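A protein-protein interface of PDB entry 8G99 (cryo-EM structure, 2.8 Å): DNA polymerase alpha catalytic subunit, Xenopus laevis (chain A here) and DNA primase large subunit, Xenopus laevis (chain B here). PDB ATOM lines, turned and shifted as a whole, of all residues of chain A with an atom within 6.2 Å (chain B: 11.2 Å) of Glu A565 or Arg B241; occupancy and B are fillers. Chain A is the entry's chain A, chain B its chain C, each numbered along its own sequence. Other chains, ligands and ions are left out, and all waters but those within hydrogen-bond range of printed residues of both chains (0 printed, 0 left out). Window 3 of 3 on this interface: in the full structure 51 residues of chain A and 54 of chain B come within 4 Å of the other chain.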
ATOM      1  N   THR A 546       3.338   6.166   2.680  1.00  0.00           N
ATOM      2  CA  THR A 546       3.010   5.154   1.685  1.00  0.00           C
ATOM      3  C   THR A 546       4.198   4.307   1.254  1.00  0.00           C
ATOM      4  O   THR A 546       4.000   3.325   0.534  1.00  0.00           O
ATOM      5  CB  THR A 546       2.401   5.812   0.439  1.00  0.00           C
ATOM      6  OG1 THR A 546       3.357   6.698  -0.154  1.00  0.00           O
ATOM      7  CG2 THR A 546       1.149   6.587   0.798  1.00  0.00           C
ATOM      8  N   VAL A 547       5.412   4.642   1.680  1.00  0.00           N
ATOM      9  CA  VAL A 547       6.620   3.949   1.250  1.00  0.00           C
ATOM     10  C   VAL A 547       7.283   3.328   2.469  1.00  0.00           C
ATOM     11  O   VAL A 547       7.512   4.011   3.474  1.00  0.00           O
ATOM     12  CB  VAL A 547       7.590   4.901   0.528  1.00  0.00           C
ATOM     13  CG1 VAL A 547       8.974   4.284   0.430  1.00  0.00           C
ATOM     14  CG2 VAL A 547       7.063   5.247  -0.852  1.00  0.00           C
ATOM     15  N   HIS A 548       7.588   2.038   2.378  1.00  0.00           N
ATOM     16  CA  HIS A 548       8.284   1.343   3.448  1.00  0.00           C
ATOM     17  C   HIS A 548       9.772   1.656   3.395  1.00  0.00           C
ATOM     18  O   HIS A 548      10.371   1.718   2.318  1.00  0.00           O
ATOM     19  CB  HIS A 548       8.061  -0.165   3.343  1.00  0.00           C
ATOM     20  CG  HIS A 548       6.618  -0.561   3.336  1.00  0.00           C
ATOM     21  ND1 HIS A 548       5.768  -0.260   2.294  1.00  0.00           N
ATOM     22  CD2 HIS A 548       5.874  -1.236   4.243  1.00  0.00           C
ATOM     23  CE1 HIS A 548       4.564  -0.732   2.560  1.00  0.00           C
ATOM     24  NE2 HIS A 548       4.601  -1.328   3.738  1.00  0.00           N
ATOM     25  N   GLU A 562      19.375   0.532  -0.649  1.00  0.00           N
ATOM     26  CA  GLU A 562      18.262  -0.076  -1.365  1.00  0.00           C
ATOM     27  C   GLU A 562      17.149   0.940  -1.593  1.00  0.00           C
ATOM     28  O   GLU A 562      16.810   1.710  -0.696  1.00  0.00           O
ATOM     29  CB  GLU A 562      17.722  -1.281  -0.593  1.00  0.00           C
ATOM     30  CG  GLU A 562      18.720  -2.417  -0.442  1.00  0.00           C
ATOM     31  CD  GLU A 562      18.182  -3.560   0.397  1.00  0.00           C
ATOM     32  OE1 GLU A 562      17.113  -3.389   1.020  1.00  0.00           O
ATOM     33  OE2 GLU A 562      18.827  -4.628   0.433  1.00  0.00           O
ATOM     34  N   ILE A 563      16.586   0.937  -2.796  1.00  0.00           N
ATOM     35  CA  ILE A 563      15.513   1.856  -3.162  1.00  0.00           C
ATOM     36  C   ILE A 563      14.184   1.163  -2.868  1.00  0.00           C
ATOM     37  O   ILE A 563      13.947   0.066  -3.395  1.00  0.00           O
ATOM     38  CB  ILE A 563      15.598   2.272  -4.634  1.00  0.00           C
ATOM     39  CG1 ILE A 563      17.057   2.366  -5.094  1.00  0.00           C
ATOM     40  CG2 ILE A 563      14.888   3.598  -4.851  1.00  0.00           C
ATOM     41  CD1 ILE A 563      17.923   3.269  -4.243  1.00  0.00           C
ATOM     42  N   PRO A 564      13.309   1.748  -2.052  1.00  0.00           N
ATOM     43  CA  PRO A 564      12.052   1.069  -1.724  1.00  0.00           C
ATOM     44  C   PRO A 564      11.165   0.904  -2.948  1.00  0.00           C
ATOM     45  O   PRO A 564      11.211   1.698  -3.889  1.00  0.00           O
ATOM     46  CB  PRO A 564      11.409   1.994  -0.687  1.00  0.00           C
ATOM     47  CG  PRO A 564      11.992   3.330  -0.960  1.00  0.00           C
ATOM     48  CD  PRO A 564      13.388   3.085  -1.442  1.00  0.00           C
ATOM     49  N   GLU A 565      10.353  -0.147  -2.926  1.00  0.00           N
ATOM     50  CA  GLU A 565       9.432  -0.403  -4.019  1.00  0.00           C
ATOM     51  C   GLU A 565       8.302   0.622  -4.018  1.00  0.00           C
ATOM     52  O   GLU A 565       7.964   1.218  -2.991  1.00  0.00           O
ATOM     53  CB  GLU A 565       8.858  -1.816  -3.916  1.00  0.00           C
ATOM     54  CG  GLU A 565       8.493  -2.433  -5.257  1.00  0.00           C
ATOM     55  CD  GLU A 565       7.846  -3.797  -5.114  1.00  0.00           C
ATOM     56  OE1 GLU A 565       7.568  -4.208  -3.969  1.00  0.00           O
ATOM     57  OE2 GLU A 565       7.615  -4.457  -6.150  1.00  0.00           O
ATOM     58  N   LEU A 566       7.714   0.821  -5.190  1.00  0.00           N
ATOM     59  CA  LEU A 566       6.652   1.803  -5.326  1.00  0.00           C
ATOM     60  C   LEU A 566       5.429   1.375  -4.517  1.00  0.00           C
ATOM     61  O   LEU A 566       5.136   0.179  -4.419  1.00  0.00           O
ATOM     62  CB  LEU A 566       6.267   1.970  -6.794  1.00  0.00           C
ATOM     63  CG  LEU A 566       7.331   2.594  -7.693  1.00  0.00           C
ATOM     64  CD1 LEU A 566       7.095   2.211  -9.144  1.00  0.00           C
ATOM     65  CD2 LEU A 566       7.344   4.100  -7.530  1.00  0.00           C
ATOM     66  N   PRO A 567       4.697   2.318  -3.924  1.00  0.00           N
ATOM     67  CA  PRO A 567       3.473   1.948  -3.209  1.00  0.00           C
ATOM     68  C   PRO A 567       2.431   1.360  -4.146  1.00  0.00           C
ATOM     69  O   PRO A 567       2.335   1.730  -5.317  1.00  0.00           O
ATOM     70  CB  PRO A 567       2.995   3.274  -2.604  1.00  0.00           C
ATOM     71  CG  PRO A 567       3.695   4.331  -3.362  1.00  0.00           C
ATOM     72  CD  PRO A 567       4.990   3.754  -3.807  1.00  0.00           C
ATOM     73  N   LEU A 640      14.141   6.895  -4.416  1.00  0.00           N
ATOM     74  CA  LEU A 640      13.061   6.420  -5.272  1.00  0.00           C
ATOM     75  C   LEU A 640      12.645   7.489  -6.273  1.00  0.00           C
ATOM     76  O   LEU A 640      12.436   7.197  -7.459  1.00  0.00           O
ATOM     77  CB  LEU A 640      11.872   5.993  -4.412  1.00  0.00           C
ATOM     78  CG  LEU A 640      10.671   5.404  -5.149  1.00  0.00           C
ATOM     79  CD1 LEU A 640      11.076   4.179  -5.949  1.00  0.00           C
ATOM     80  CD2 LEU A 640       9.572   5.063  -4.166  1.00  0.00           C
ATOM     81  N   HIS A 643      15.284   7.762  -8.974  1.00  0.00           N
ATOM     82  CA  HIS A 643      15.233   6.626  -9.890  1.00  0.00           C
ATOM     83  C   HIS A 643      14.078   6.768 -10.874  1.00  0.00           C
ATOM     84  O   HIS A 643      14.238   6.535 -12.084  1.00  0.00           O
ATOM     85  CB  HIS A 643      15.111   5.333  -9.083  1.00  0.00           C
ATOM     86  CG  HIS A 643      14.903   4.109  -9.915  1.00  0.00           C
ATOM     87  ND1 HIS A 643      13.653   3.619 -10.217  1.00  0.00           N
ATOM     88  CD2 HIS A 643      15.788   3.261 -10.489  1.00  0.00           C
ATOM     89  CE1 HIS A 643      13.774   2.531 -10.955  1.00  0.00           C
ATOM     90  NE2 HIS A 643      15.060   2.292 -11.134  1.00  0.00           N
ATOM     91  N   GLN A 644      12.909   7.174 -10.381  1.00  0.00           N
ATOM     92  CA  GLN A 644      11.774   7.375 -11.274  1.00  0.00           C
ATOM     93  C   GLN A 644      12.047   8.504 -12.259  1.00  0.00           C
ATOM     94  O   GLN A 644      11.655   8.428 -13.429  1.00  0.00           O
ATOM     95  CB  GLN A 644      10.511   7.654 -10.464  1.00  0.00           C
ATOM     96  CG  GLN A 644      10.041   6.475  -9.632  1.00  0.00           C
ATOM     97  CD  GLN A 644       9.754   5.246 -10.467  1.00  0.00           C
ATOM     98  OE1 GLN A 644      10.614   4.383 -10.638  1.00  0.00           O
ATOM     99  NE2 GLN A 644       8.541   5.161 -10.993  1.00  0.00           N
ATOM    100  N   ARG B 113      22.512  -7.919 -18.218  1.00  0.00           N
ATOM    101  CA  ARG B 113      21.583  -7.364 -17.243  1.00  0.00           C
ATOM    102  C   ARG B 113      21.996  -5.948 -16.891  1.00  0.00           C
ATOM    103  O   ARG B 113      21.191  -5.012 -16.962  1.00  0.00           O
ATOM    104  CB  ARG B 113      21.545  -8.234 -15.987  1.00  0.00           C
ATOM    105  CG  ARG B 113      20.472  -9.291 -15.973  1.00  0.00           C
ATOM    106  CD  ARG B 113      20.310  -9.848 -14.576  1.00  0.00           C
ATOM    107  NE  ARG B 113      19.802 -11.213 -14.576  1.00  0.00           N
ATOM    108  CZ  ARG B 113      19.714 -11.975 -13.495  1.00  0.00           C
ATOM    109  NH1 ARG B 113      20.087 -11.533 -12.306  1.00  0.00           N
ATOM    110  NH2 ARG B 113      19.242 -13.211 -13.611  1.00  0.00           N
ATOM    111  N   LEU B 114      23.272  -5.770 -16.560  1.00  0.00           N
ATOM    112  CA  LEU B 114      23.769  -4.432 -16.271  1.00  0.00           C
ATOM    113  C   LEU B 114      23.536  -3.500 -17.447  1.00  0.00           C
ATOM    114  O   LEU B 114      23.292  -2.305 -17.256  1.00  0.00           O
ATOM    115  CB  LEU B 114      25.255  -4.480 -15.920  1.00  0.00           C
ATOM    116  CG  LEU B 114      25.591  -4.688 -14.445  1.00  0.00           C
ATOM    117  CD1 LEU B 114      27.080  -4.915 -14.279  1.00  0.00           C
ATOM    118  CD2 LEU B 114      25.134  -3.506 -13.610  1.00  0.00           C
ATOM    119  N   TYR B 116      20.989  -3.816 -19.639  1.00  0.00           N
ATOM    120  CA  TYR B 116      19.595  -3.757 -20.069  1.00  0.00           C
ATOM    121  C   TYR B 116      18.635  -3.597 -18.898  1.00  0.00           C
ATOM    122  O   TYR B 116      17.619  -4.296 -18.821  1.00  0.00           O
ATOM    123  CB  TYR B 116      19.244  -5.016 -20.868  1.00  0.00           C
ATOM    124  CG  TYR B 116      19.582  -4.928 -22.335  1.00  0.00           C
ATOM    125  CD1 TYR B 116      18.689  -4.382 -23.242  1.00  0.00           C
ATOM    126  CD2 TYR B 116      20.793  -5.397 -22.816  1.00  0.00           C
ATOM    127  CE1 TYR B 116      18.995  -4.301 -24.582  1.00  0.00           C
ATOM    128  CE2 TYR B 116      21.106  -5.319 -24.154  1.00  0.00           C
ATOM    129  CZ  TYR B 116      20.204  -4.770 -25.032  1.00  0.00           C
ATOM    130  OH  TYR B 116      20.513  -4.691 -26.368  1.00  0.00           O
ATOM    131  N   CYS B 117      18.943  -2.686 -17.980  1.00  0.00           N
ATOM    132  CA  CYS B 117      18.072  -2.411 -16.850  1.00  0.00           C
ATOM    133  C   CYS B 117      17.781  -0.930 -16.668  1.00  0.00           C
ATOM    134  O   CYS B 117      17.071  -0.567 -15.725  1.00  0.00           O
ATOM    135  CB  CYS B 117      18.684  -2.967 -15.556  1.00  0.00           C
ATOM    136  SG  CYS B 117      20.357  -2.386 -15.214  1.00  0.00           S
ATOM    137  N   GLN B 118      18.303  -0.066 -17.538  1.00  0.00           N
ATOM    138  CA  GLN B 118      18.159   1.370 -17.342  1.00  0.00           C
ATOM    139  C   GLN B 118      16.757   1.857 -17.689  1.00  0.00           C
ATOM    140  O   GLN B 118      16.223   2.738 -17.008  1.00  0.00           O
ATOM    141  CB  GLN B 118      19.200   2.110 -18.179  1.00  0.00           C
ATOM    142  CG  GLN B 118      20.596   2.078 -17.583  1.00  0.00           C
ATOM    143  CD  GLN B 118      21.652   1.633 -18.575  1.00  0.00           C
ATOM    144  OE1 GLN B 118      21.482   1.767 -19.786  1.00  0.00           O
ATOM    145  NE2 GLN B 118      22.756   1.101 -18.061  1.00  0.00           N
ATOM    146  N   SER B 119      16.149   1.304 -18.734  1.00  0.00           N
ATOM    147  CA  SER B 119      14.860   1.771 -19.223  1.00  0.00           C
ATOM    148  C   SER B 119      13.913   0.597 -19.399  1.00  0.00           C
ATOM    149  O   SER B 119      14.315  -0.475 -19.862  1.00  0.00           O
ATOM    150  CB  SER B 119      15.012   2.516 -20.552  1.00  0.00           C
ATOM    151  OG  SER B 119      14.708   1.669 -21.646  1.00  0.00           O
ATOM    152  N   GLU B 120      12.643   0.820 -19.053  1.00  0.00           N
ATOM    153  CA  GLU B 120      11.648  -0.241 -19.137  1.00  0.00           C
ATOM    154  C   GLU B 120      11.662  -0.897 -20.509  1.00  0.00           C
ATOM    155  O   GLU B 120      11.714  -2.127 -20.619  1.00  0.00           O
ATOM    156  CB  GLU B 120      10.260   0.322 -18.826  1.00  0.00           C
ATOM    157  CG  GLU B 120       9.140  -0.707 -18.887  1.00  0.00           C
ATOM    158  CD  GLU B 120       9.379  -1.892 -17.972  1.00  0.00           C
ATOM    159  OE1 GLU B 120       9.826  -1.679 -16.825  1.00  0.00           O
ATOM    160  OE2 GLU B 120       9.120  -3.036 -18.399  1.00  0.00           O
ATOM    161  N   ARG B 123      14.446  -3.213 -20.716  1.00  0.00           N
ATOM    162  CA  ARG B 123      14.193  -4.376 -19.880  1.00  0.00           C
ATOM    163  C   ARG B 123      13.332  -5.371 -20.631  1.00  0.00           C
ATOM    164  O   ARG B 123      13.720  -6.530 -20.817  1.00  0.00           O
ATOM    165  CB  ARG B 123      13.510  -3.953 -18.580  1.00  0.00           C
ATOM    166  CG  ARG B 123      14.401  -3.183 -17.632  1.00  0.00           C
ATOM    167  CD  ARG B 123      13.888  -3.252 -16.207  1.00  0.00           C
ATOM    168  NE  ARG B 123      12.816  -2.294 -15.967  1.00  0.00           N
ATOM    169  CZ  ARG B 123      13.004  -1.007 -15.715  1.00  0.00           C
ATOM    170  NH1 ARG B 123      14.216  -0.480 -15.666  1.00  0.00           N
ATOM    171  NH2 ARG B 123      11.947  -0.227 -15.507  1.00  0.00           N
ATOM    172  N   ALA B 230       9.174 -14.408 -14.196  1.00  0.00           N
ATOM    173  CA  ALA B 230       9.010 -13.753 -12.909  1.00  0.00           C
ATOM    174  C   ALA B 230      10.381 -13.386 -12.371  1.00  0.00           C
ATOM    175  O   ALA B 230      10.735 -12.199 -12.238  1.00  0.00           O
ATOM    176  CB  ALA B 230       8.259 -14.668 -11.940  1.00  0.00           C
ATOM    177  N   LEU B 232      13.278 -13.174 -13.627  1.00  0.00           N
ATOM    178  CA  LEU B 232      14.112 -12.266 -14.394  1.00  0.00           C
ATOM    179  C   LEU B 232      13.650 -10.840 -14.189  1.00  0.00           C
ATOM    180  O   LEU B 232      14.466  -9.941 -13.960  1.00  0.00           O
ATOM    181  CB  LEU B 232      14.078 -12.641 -15.875  1.00  0.00           C
ATOM    182  CG  LEU B 232      15.394 -12.463 -16.631  1.00  0.00           C
ATOM    183  CD1 LEU B 232      15.329 -13.153 -17.978  1.00  0.00           C
ATOM    184  CD2 LEU B 232      15.723 -10.990 -16.799  1.00  0.00           C
ATOM    185  N   SER B 233      12.340 -10.619 -14.234  1.00  0.00           N
ATOM    186  CA  SER B 233      11.831  -9.274 -14.017  1.00  0.00           C
ATOM    187  C   SER B 233      12.305  -8.759 -12.673  1.00  0.00           C
ATOM    188  O   SER B 233      12.881  -7.664 -12.573  1.00  0.00           O
ATOM    189  CB  SER B 233      10.305  -9.265 -14.099  1.00  0.00           C
ATOM    190  OG  SER B 233       9.844 -10.108 -15.139  1.00  0.00           O
ATOM    191  N   LYS B 234      12.116  -9.568 -11.628  1.00  0.00           N
ATOM    192  CA  LYS B 234      12.565  -9.139 -10.311  1.00  0.00           C
ATOM    193  C   LYS B 234      14.028  -8.731 -10.384  1.00  0.00           C
ATOM    194  O   LYS B 234      14.412  -7.629  -9.962  1.00  0.00           O
ATOM    195  CB  LYS B 234      12.355 -10.258  -9.292  1.00  0.00           C
ATOM    196  CG  LYS B 234      11.638  -9.817  -8.027  1.00  0.00           C
ATOM    197  CD  LYS B 234      11.001 -10.997  -7.307  1.00  0.00           C
ATOM    198  CE  LYS B 234       9.688 -11.421  -7.951  1.00  0.00           C
ATOM    199  NZ  LYS B 234       8.670 -10.333  -7.947  1.00  0.00           N
ATOM    200  N   ALA B 235      14.843  -9.592 -10.994  1.00  0.00           N
ATOM    201  CA  ALA B 235      16.273  -9.341 -11.029  1.00  0.00           C
ATOM    202  C   ALA B 235      16.551  -8.014 -11.702  1.00  0.00           C
ATOM    203  O   ALA B 235      17.334  -7.205 -11.196  1.00  0.00           O
ATOM    204  CB  ALA B 235      16.990 -10.478 -11.754  1.00  0.00           C
ATOM    205  N   LEU B 236      15.881  -7.756 -12.821  1.00  0.00           N
ATOM    206  CA  LEU B 236      16.137  -6.523 -13.543  1.00  0.00           C
ATOM    207  C   LEU B 236      15.799  -5.332 -12.669  1.00  0.00           C
ATOM    208  O   LEU B 236      16.559  -4.358 -12.611  1.00  0.00           O
ATOM    209  CB  LEU B 236      15.339  -6.495 -14.845  1.00  0.00           C
ATOM    210  CG  LEU B 236      15.921  -7.350 -15.970  1.00  0.00           C
ATOM    211  CD1 LEU B 236      14.884  -7.596 -17.044  1.00  0.00           C
ATOM    212  CD2 LEU B 236      17.154  -6.697 -16.561  1.00  0.00           C
ATOM    213  N   ALA B 237      14.678  -5.408 -11.953  1.00  0.00           N
ATOM    214  CA  ALA B 237      14.350  -4.323 -11.040  1.00  0.00           C
ATOM    215  C   ALA B 237      15.514  -4.094 -10.091  1.00  0.00           C
ATOM    216  O   ALA B 237      16.040  -2.978  -9.971  1.00  0.00           O
ATOM    217  CB  ALA B 237      13.069  -4.646 -10.271  1.00  0.00           C
ATOM    218  N   LEU B 238      15.983  -5.173  -9.465  1.00  0.00           N
ATOM    219  CA  LEU B 238      17.071  -5.026  -8.508  1.00  0.00           C
ATOM    220  C   LEU B 238      18.272  -4.375  -9.172  1.00  0.00           C
ATOM    221  O   LEU B 238      18.915  -3.492  -8.591  1.00  0.00           O
ATOM    222  CB  LEU B 238      17.443  -6.383  -7.915  1.00  0.00           C
ATOM    223  CG  LEU B 238      16.920  -6.614  -6.497  1.00  0.00           C
ATOM    224  CD1 LEU B 238      15.404  -6.562  -6.474  1.00  0.00           C
ATOM    225  CD2 LEU B 238      17.421  -7.941  -5.950  1.00  0.00           C
ATOM    226  N   SER B 239      18.565  -4.772 -10.410  1.00  0.00           N
ATOM    227  CA  SER B 239      19.725  -4.222 -11.095  1.00  0.00           C
ATOM    228  C   SER B 239      19.556  -2.727 -11.295  1.00  0.00           C
ATOM    229  O   SER B 239      20.489  -1.949 -11.067  1.00  0.00           O
ATOM    230  CB  SER B 239      19.928  -4.929 -12.433  1.00  0.00           C
ATOM    231  OG  SER B 239      21.047  -4.403 -13.124  1.00  0.00           O
ATOM    232  N   ALA B 240      18.358  -2.307 -11.692  1.00  0.00           N
ATOM    233  CA  ALA B 240      18.104  -0.886 -11.870  1.00  0.00           C
ATOM    234  C   ALA B 240      18.258  -0.149 -10.553  1.00  0.00           C
ATOM    235  O   ALA B 240      18.603   1.037 -10.539  1.00  0.00           O
ATOM    236  CB  ALA B 240      16.708  -0.666 -12.451  1.00  0.00           C
ATOM    237  N   ARG B 241      18.014  -0.837  -9.436  1.00  0.00           N
ATOM    238  CA  ARG B 241      18.196  -0.206  -8.137  1.00  0.00           C
ATOM    239  C   ARG B 241      19.665  -0.074  -7.753  1.00  0.00           C
ATOM    240  O   ARG B 241      19.992   0.753  -6.897  1.00  0.00           O
ATOM    241  CB  ARG B 241      17.447  -0.995  -7.063  1.00  0.00           C
ATOM    242  CG  ARG B 241      16.059  -0.458  -6.771  1.00  0.00           C
ATOM    243  CD  ARG B 241      15.059  -0.871  -7.831  1.00  0.00           C
ATOM    244  NE  ARG B 241      13.943   0.063  -7.915  1.00  0.00           N
ATOM    245  CZ  ARG B 241      12.923   0.093  -7.069  1.00  0.00           C
ATOM    246  NH1 ARG B 241      12.844  -0.745  -6.049  1.00  0.00           N
ATOM    247  NH2 ARG B 241      11.956   0.987  -7.252  1.00  0.00           N
ATOM    248  N   SER B 242      20.553  -0.863  -8.360  1.00  0.00           N
ATOM    249  CA  SER B 242      21.970  -0.862  -8.020  1.00  0.00           C
ATOM    250  C   SER B 242      22.826  -0.259  -9.130  1.00  0.00           C
ATOM    251  O   SER B 242      23.983  -0.644  -9.310  1.00  0.00           O
ATOM    252  CB  SER B 242      22.439  -2.281  -7.706  1.00  0.00           C
ATOM    253  OG  SER B 242      22.192  -3.153  -8.796  1.00  0.00           O
ATOM    254  N   LEU B 243      22.270   0.688  -9.879  1.00  0.00           N
ATOM    255  CA  LEU B 243      22.957   1.292 -11.014  1.00  0.00           C
ATOM    256  C   LEU B 243      23.995   2.322 -10.584  1.00  0.00           C
ATOM    257  O   LEU B 243      25.069   2.394 -11.191  1.00  0.00           O
ATOM    258  CB  LEU B 243      21.945   1.944 -11.958  1.00  0.00           C
ATOM    259  CG  LEU B 243      22.279   1.860 -13.447  1.00  0.00           C
ATOM    260  CD1 LEU B 243      22.275   0.417 -13.929  1.00  0.00           C
ATOM    261  CD2 LEU B 243      21.303   2.694 -14.255  1.00  0.00           C
ATOM    262  N   PRO B 244      23.723   3.140  -9.562  1.00  0.00           N
ATOM    263  CA  PRO B 244      24.702   4.175  -9.191  1.00  0.00           C
ATOM    264  C   PRO B 244      26.077   3.625  -8.865  1.00  0.00           C
ATOM    265  O   PRO B 244      27.076   4.323  -9.074  1.00  0.00           O
ATOM    266  CB  PRO B 244      24.054   4.839  -7.970  1.00  0.00           C
ATOM    267  CG  PRO B 244      22.599   4.644  -8.173  1.00  0.00           C
ATOM    268  CD  PRO B 244      22.455   3.302  -8.828  1.00  0.00           C
ATOM    269  N   VAL B 245      26.166   2.395  -8.358  1.00  0.00           N
ATOM    270  CA  VAL B 245      27.463   1.825  -8.018  1.00  0.00           C
ATOM    271  C   VAL B 245      28.303   1.534  -9.255  1.00  0.00           C
ATOM    272  O   VAL B 245      29.531   1.433  -9.152  1.00  0.00           O
ATOM    273  CB  VAL B 245      27.275   0.543  -7.185  1.00  0.00           C
ATOM    274  CG1 VAL B 245      28.626  -0.059  -6.816  1.00  0.00           C
ATOM    275  CG2 VAL B 245      26.458   0.836  -5.934  1.00  0.00           C
ATOM    276  N   VAL B 246      27.684   1.404 -10.426  1.00  0.00           N
ATOM    277  CA  VAL B 246      28.392   0.983 -11.630  1.00  0.00           C
ATOM    278  C   VAL B 246      28.760   2.191 -12.481  1.00  0.00           C
ATOM    279  O   VAL B 246      29.785   2.187 -13.170  1.00  0.00           O
ATOM    280  CB  VAL B 246      27.547  -0.015 -12.440  1.00  0.00           C
ATOM    281  CG1 VAL B 246      28.234  -0.353 -13.755  1.00  0.00           C
ATOM    282  CG2 VAL B 246      27.293  -1.271 -11.624  1.00  0.00           C
ATOM    283  N   GLN B 247      27.928   3.233 -12.438  1.00  0.00           N
ATOM    284  CA  GLN B 247      28.176   4.406 -13.268  1.00  0.00           C
ATOM    285  C   GLN B 247      29.524   5.041 -12.956  1.00  0.00           C
ATOM    286  O   GLN B 247      30.123   5.682 -13.825  1.00  0.00           O
ATOM    287  CB  GLN B 247      27.054   5.425 -13.083  1.00  0.00           C
ATOM    288  CG  GLN B 247      26.831   6.324 -14.287  1.00  0.00           C
ATOM    289  CD  GLN B 247      26.200   7.651 -13.915  1.00  0.00           C
ATOM    290  OE1 GLN B 247      26.879   8.568 -13.452  1.00  0.00           O
ATOM    291  NE2 GLN B 247      24.892   7.763 -14.118  1.00  0.00           N
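NH1 of Arg B241 sits at hydrogen-bond distance from O of Ile A563 (3.0 Å).
Hydrophobic or aromatic side chains of chain B within 4 Å of the printed part of chain A: Ala B240. Of the 12 printed residues of chain A, 5 touch a printed residue of chain B. Among the printed residues, 6 pairs touch across the chains.
Arg B241 touches Pro A564. NH1 of Arg B241 touches CA of Glu A565, at 3.98 Å. Arg B241 touches Leu A640 (NH2 to CD1, 3.6 Å). CD2 of His A643 touches O of Ala B240, at 3.6 Å. CE1 of His A643 touches NE of Arg B241 (3.9 Å).
A ring nitrogen (ND1) of His A643 is in hydrogen-bond range of the side-chain amide oxygen (OE1) of Gln A644, at 3.2 Å.
Pro A564 touches just one residue of chain B: Arg B241 (3.5 Å). Printed residues of chain B within 4 Å of Glu A565: Arg B241 (3.98 Å). No residue of chain B comes within 4 Å of Leu A566. No residue of chain B comes within 4 Å of Pro A567. Leu A640 touches just one residue of chain B: Arg B241. Of the printed residues of chain B, His A643 touches Ala B240 and Arg B241. Tyr B116 touches none of the printed residues of chain A. Of the printed residues of chain A, Ala B240 touches His A643 (3.6 Å). Of the printed residues of chain A, Arg B241 touches Ile A563 (3.0 Å), Pro A564 (3.5 Å), Glu A565 (3.98 Å), Leu A640 (3.6 Å) and His A643 (3.9 Å). The nearest printed residue of chain B that does not touch Glu A565 is Lys B234 (6.2 Å).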
